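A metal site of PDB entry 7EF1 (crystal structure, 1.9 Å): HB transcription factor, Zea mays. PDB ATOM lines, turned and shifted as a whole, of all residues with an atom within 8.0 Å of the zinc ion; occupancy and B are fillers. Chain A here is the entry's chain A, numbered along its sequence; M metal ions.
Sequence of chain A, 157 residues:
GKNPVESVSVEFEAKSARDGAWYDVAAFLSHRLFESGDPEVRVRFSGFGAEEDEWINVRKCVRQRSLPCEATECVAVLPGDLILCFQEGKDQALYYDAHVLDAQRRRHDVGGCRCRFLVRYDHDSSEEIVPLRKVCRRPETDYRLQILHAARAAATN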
ATOM      1  N   GLU A  70     -14.783  -0.737  12.921  1.00  0.00           N
ATOM      2  CA  GLU A  70     -14.075  -0.948  11.661  1.00  0.00           C
ATOM      3  C   GLU A  70     -12.946   0.064  11.531  1.00  0.00           C
ATOM      4  O   GLU A  70     -13.033   1.164  12.095  1.00  0.00           O
ATOM      5  CB  GLU A  70     -15.026  -0.806  10.460  1.00  0.00           C
ATOM      6  CG  GLU A  70     -16.150  -1.832  10.375  1.00  0.00           C
ATOM      7  CD  GLU A  70     -15.747  -3.092   9.622  1.00  0.00           C
ATOM      8  OE1 GLU A  70     -14.689  -3.102   8.962  1.00  0.00           O
ATOM      9  OE2 GLU A  70     -16.504  -4.088   9.703  1.00  0.00           O
ATOM     10  N   ALA A  71     -11.904  -0.299  10.795  1.00  0.00           N
ATOM     11  CA  ALA A  71     -10.693   0.514  10.698  1.00  0.00           C
ATOM     12  C   ALA A  71     -10.980   1.944  10.260  1.00  0.00           C
ATOM     13  O   ALA A  71     -10.351   2.883  10.750  1.00  0.00           O
ATOM     14  CB  ALA A  71      -9.693  -0.145   9.752  1.00  0.00           C
ATOM     15  N   THR A  72     -11.934   2.107   9.351  1.00  0.00           N
ATOM     16  CA  THR A  72     -12.263   3.418   8.812  1.00  0.00           C
ATOM     17  C   THR A  72     -13.148   4.233   9.750  1.00  0.00           C
ATOM     18  O   THR A  72     -13.337   5.436   9.539  1.00  0.00           O
ATOM     19  CB  THR A  72     -12.967   3.295   7.455  1.00  0.00           C
ATOM     20  OG1 THR A  72     -13.445   4.575   7.039  1.00  0.00           O
ATOM     21  CG2 THR A  72     -14.141   2.332   7.562  1.00  0.00           C
ATOM     22  N   GLU A  73     -13.677   3.603  10.781  1.00  0.00           N
ATOM     23  CA  GLU A  73     -14.675   4.245  11.631  1.00  0.00           C
ATOM     24  C   GLU A  73     -14.068   5.038  12.796  1.00  0.00           C
ATOM     25  O   GLU A  73     -14.794   5.590  13.625  1.00  0.00           O
ATOM     26  CB  GLU A  73     -15.654   3.193  12.148  1.00  0.00           C
ATOM     27  CG  GLU A  73     -16.479   2.543  11.038  1.00  0.00           C
ATOM     28  CD  GLU A  73     -17.413   1.455  11.551  1.00  0.00           C
ATOM     29  OE1 GLU A  73     -17.182   0.947  12.676  1.00  0.00           O
ATOM     30  OE2 GLU A  73     -18.370   1.112  10.825  1.00  0.00           O
ATOM     31  N   CYS A  74     -12.746   5.112  12.843  1.00  0.00           N
ATOM     32  CA  CYS A  74     -12.069   5.900  13.866  1.00  0.00           C
ATOM     33  C   CYS A  74     -12.483   7.380  13.795  1.00  0.00           C
ATOM     34  O   CYS A  74     -12.409   8.095  14.781  1.00  0.00           O
ATOM     35  CB  CYS A  74     -10.557   5.768  13.743  1.00  0.00           C
ATOM     36  SG  CYS A  74      -9.892   6.211  12.136  1.00  0.00           S
ATOM     37  N   VAL A  75     -12.950   7.827  12.630  1.00  0.00           N
ATOM     38  CA  VAL A  75     -13.357   9.220  12.471  1.00  0.00           C
ATOM     39  C   VAL A  75     -14.670   9.502  13.196  1.00  0.00           C
ATOM     40  O   VAL A  75     -15.039  10.656  13.390  1.00  0.00           O
ATOM     41  CB  VAL A  75     -13.493   9.604  10.975  1.00  0.00           C
ATOM     42  CG1 VAL A  75     -12.185   9.392  10.240  1.00  0.00           C
ATOM     43  CG2 VAL A  75     -14.600   8.808  10.318  1.00  0.00           C
ATOM     44  N   GLN A 104      -5.215  10.813  19.025  1.00  0.00           N
ATOM     45  CA  GLN A 104      -4.027  11.017  18.223  1.00  0.00           C
ATOM     46  C   GLN A 104      -4.243  10.303  16.901  1.00  0.00           C
ATOM     47  O   GLN A 104      -4.159   9.071  16.838  1.00  0.00           O
ATOM     48  CB  GLN A 104      -2.783  10.507  18.934  1.00  0.00           C
ATOM     49  CG  GLN A 104      -1.489  10.766  18.181  1.00  0.00           C
ATOM     50  CD  GLN A 104      -0.302  10.072  18.815  1.00  0.00           C
ATOM     51  OE1 GLN A 104      -0.288   8.845  18.964  1.00  0.00           O
ATOM     52  NE2 GLN A 104       0.710  10.851  19.198  1.00  0.00           N
ATOM     53  N   ARG A 105      -4.547  11.052  15.856  1.00  0.00           N
ATOM     54  CA  ARG A 105      -4.930  10.438  14.588  1.00  0.00           C
ATOM     55  C   ARG A 105      -3.724  10.348  13.672  1.00  0.00           C
ATOM     56  O   ARG A 105      -3.042  11.346  13.409  1.00  0.00           O
ATOM     57  CB  ARG A 105      -6.069  11.220  13.955  1.00  0.00           C
ATOM     58  CG  ARG A 105      -7.220  11.459  14.925  1.00  0.00           C
ATOM     59  CD  ARG A 105      -8.453  12.055  14.270  1.00  0.00           C
ATOM     60  NE  ARG A 105      -9.467  12.371  15.273  1.00  0.00           N
ATOM     61  CZ  ARG A 105     -10.395  11.535  15.708  1.00  0.00           C
ATOM     62  NH1 ARG A 105     -10.457  10.290  15.224  1.00  0.00           N
ATOM     63  NH2 ARG A 105     -11.265  11.919  16.623  1.00  0.00           N
ATOM     64  N   ARG A 106      -3.443   9.135  13.202  1.00  0.00           N
ATOM     65  CA  ARG A 106      -2.282   8.870  12.369  1.00  0.00           C
ATOM     66  C   ARG A 106      -2.697   8.126  11.110  1.00  0.00           C
ATOM     67  O   ARG A 106      -3.691   7.395  11.116  1.00  0.00           O
ATOM     68  CB  ARG A 106      -1.238   8.066  13.147  1.00  0.00           C
ATOM     69  CG  ARG A 106      -0.921   8.637  14.529  1.00  0.00           C
ATOM     70  CD  ARG A 106       0.176   7.851  15.247  1.00  0.00           C
ATOM     71  NE  ARG A 106      -0.243   6.488  15.563  1.00  0.00           N
ATOM     72  CZ  ARG A 106       0.482   5.645  16.300  1.00  0.00           C
ATOM     73  NH1 ARG A 106       1.649   6.018  16.802  1.00  0.00           N
ATOM     74  NH2 ARG A 106       0.030   4.419  16.532  1.00  0.00           N
ATOM     75  N   ARG A 107      -1.958   8.308  10.026  1.00  0.00           N
ATOM     76  CA  ARG A 107      -2.328   7.692   8.757  1.00  0.00           C
ATOM     77  C   ARG A 107      -2.308   6.171   8.881  1.00  0.00           C
ATOM     78  O   ARG A 107      -1.434   5.584   9.530  1.00  0.00           O
ATOM     79  CB  ARG A 107      -1.396   8.154   7.623  1.00  0.00           C
ATOM     80  CG  ARG A 107       0.058   7.793   7.809  1.00  0.00           C
ATOM     81  CD  ARG A 107       0.891   8.295   6.630  1.00  0.00           C
ATOM     82  NE  ARG A 107       0.887   9.744   6.545  1.00  0.00           N
ATOM     83  CZ  ARG A 107       1.710  10.539   7.228  1.00  0.00           C
ATOM     84  NH1 ARG A 107       2.623  10.010   8.038  1.00  0.00           N
ATOM     85  NH2 ARG A 107       1.639  11.858   7.089  1.00  0.00           N
ATOM     86  N   HIS A 108      -3.302   5.534   8.269  1.00  0.00           N
ATOM     87  CA  HIS A 108      -3.450   4.089   8.344  1.00  0.00           C
ATOM     88  C   HIS A 108      -2.460   3.379   7.435  1.00  0.00           C
ATOM     89  O   HIS A 108      -1.903   3.982   6.508  1.00  0.00           O
ATOM     90  CB  HIS A 108      -4.875   3.682   7.966  1.00  0.00           C
ATOM     91  CG  HIS A 108      -5.915   4.153   8.923  1.00  0.00           C
ATOM     92  ND1 HIS A 108      -7.233   3.778   8.843  1.00  0.00           N
ATOM     93  CD2 HIS A 108      -5.830   4.987   9.989  1.00  0.00           C
ATOM     94  CE1 HIS A 108      -7.920   4.344   9.820  1.00  0.00           C
ATOM     95  NE2 HIS A 108      -7.082   5.077  10.532  1.00  0.00           N
ATOM     96  N   GLY A 112      -4.436  -1.445   8.981  1.00  0.00           N
ATOM     97  CA  GLY A 112      -5.613  -0.655   9.289  1.00  0.00           C
ATOM     98  C   GLY A 112      -5.322   0.580  10.125  1.00  0.00           C
ATOM     99  O   GLY A 112      -4.321   1.267   9.903  1.00  0.00           O
ATOM    100  N   CYS A 113      -6.204   0.849  11.085  1.00  0.00           N
ATOM    101  CA  CYS A 113      -6.156   2.087  11.863  1.00  0.00           C
ATOM    102  C   CYS A 113      -4.973   2.125  12.833  1.00  0.00           C
ATOM    103  O   CYS A 113      -4.736   1.174  13.581  1.00  0.00           O
ATOM    104  CB  CYS A 113      -7.463   2.276  12.635  1.00  0.00           C
ATOM    105  SG  CYS A 113      -7.477   3.644  13.813  1.00  0.00           S
ATOM    106  N   ARG A 114      -4.242   3.235  12.816  1.00  0.00           N
ATOM    107  CA  ARG A 114      -3.099   3.416  13.698  1.00  0.00           C
ATOM    108  C   ARG A 114      -3.359   4.528  14.718  1.00  0.00           C
ATOM    109  O   ARG A 114      -2.467   4.901  15.472  1.00  0.00           O
ATOM    110  CB  ARG A 114      -1.838   3.738  12.876  1.00  0.00           C
ATOM    111  CG  ARG A 114      -1.267   2.551  12.124  1.00  0.00           C
ATOM    112  CD  ARG A 114      -0.023   2.938  11.328  1.00  0.00           C
ATOM    113  NE  ARG A 114       0.992   3.569  12.155  1.00  0.00           N
ATOM    114  CZ  ARG A 114       1.358   4.847  12.063  1.00  0.00           C
ATOM    115  NH1 ARG A 114       0.786   5.634  11.145  1.00  0.00           N
ATOM    116  NH2 ARG A 114       2.286   5.341  12.860  1.00  0.00           N
ATOM    117  N   CYS A 115      -4.578   5.030  14.734  1.00  0.00           N
ATOM    118  CA  CYS A 115      -4.932   6.109  15.667  1.00  0.00           C
ATOM    119  C   CYS A 115      -4.890   5.607  17.102  1.00  0.00           C
ATOM    120  O   CYS A 115      -4.990   4.413  17.360  1.00  0.00           O
ATOM    121  CB  CYS A 115      -6.314   6.677  15.331  1.00  0.00           C
ATOM    122  SG  CYS A 115      -6.499   7.307  13.649  1.00  0.00           S
ATOM    123  N   ARG A 116      -4.712   6.527  18.047  1.00  0.00           N
ATOM    124  CA  ARG A 116      -4.721   6.188  19.463  1.00  0.00           C
ATOM    125  C   ARG A 116      -5.640   7.143  20.229  1.00  0.00           C
ATOM    126  O   ARG A 116      -5.729   8.325  19.901  1.00  0.00           O
ATOM    127  CB  ARG A 116      -3.307   6.224  20.038  1.00  0.00           C
ATOM    128  CG  ARG A 116      -2.318   5.316  19.323  1.00  0.00           C
ATOM    129  CD  ARG A 116      -1.048   5.175  20.135  1.00  0.00           C
ATOM    130  NE  ARG A 116      -0.591   6.452  20.647  1.00  0.00           N
ATOM    131  CZ  ARG A 116       0.319   6.593  21.610  1.00  0.00           C
ATOM    132  NH1 ARG A 116       0.669   7.805  22.013  1.00  0.00           N
ATOM    133  NH2 ARG A 116       0.862   5.517  22.164  1.00  0.00           N
ATOM    134  N   PHE A 117      -6.323   6.605  21.236  1.00  0.00           N
ATOM    135  CA  PHE A 117      -7.307   7.375  21.985  1.00  0.00           C
ATOM    136  C   PHE A 117      -7.000   7.383  23.481  1.00  0.00           C
ATOM    137  O   PHE A 117      -6.821   6.332  24.086  1.00  0.00           O
ATOM    138  CB  PHE A 117      -8.712   6.807  21.747  1.00  0.00           C
ATOM    139  CG  PHE A 117      -9.116   6.780  20.307  1.00  0.00           C
ATOM    140  CD1 PHE A 117      -8.830   5.685  19.506  1.00  0.00           C
ATOM    141  CD2 PHE A 117      -9.767   7.872  19.735  1.00  0.00           C
ATOM    142  CE1 PHE A 117      -9.188   5.663  18.163  1.00  0.00           C
ATOM    143  CE2 PHE A 117     -10.136   7.859  18.401  1.00  0.00           C
ATOM    144  CZ  PHE A 117      -9.844   6.748  17.614  1.00  0.00           C
ATOM    145  N   LEU A 132      -7.810   1.453  18.392  1.00  0.00           N
ATOM    146  CA  LEU A 132      -9.199   1.344  17.955  1.00  0.00           C
ATOM    147  C   LEU A 132      -9.783  -0.046  18.238  1.00  0.00           C
ATOM    148  O   LEU A 132     -10.976  -0.166  18.532  1.00  0.00           O
ATOM    149  CB  LEU A 132      -9.299   1.671  16.463  1.00  0.00           C
ATOM    150  CG  LEU A 132     -10.734   1.778  15.911  1.00  0.00           C
ATOM    151  CD1 LEU A 132     -11.445   3.003  16.445  1.00  0.00           C
ATOM    152  CD2 LEU A 132     -10.738   1.757  14.382  1.00  0.00           C
HETATM  153 ZN    ZN M   1      -7.677   5.625  12.557  1.00  0.00          ZN
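SG of Cys 115 lies close to N of Arg 106, 3.6 Å away.
O of Ala 71 sits close to SG of Cys 74, 3.6 Å away.
O of Cys 74 lies within hydrogen-bond range of NH1 of Arg 105 (3.0 Å).
The zinc ion is bound by a ring nitrogen (NE2) of His 108 (2.2 Å), the side-chain sulfur (SG) of Cys 115 (2.3 Å), the side-chain sulfur (SG) of Cys 74 (2.3 Å) and the side-chain sulfur (SG) of Cys 113 (2.4 Å).
The zinc ion has four donor atoms within binding distance.
Four residues have an atom within 4 Å of the zinc ion: Cys 74, His 108, Cys 113 and Cys 115.
The nearest printed residue that does not touch the zinc ion is Arg 114 (4.2 Å).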
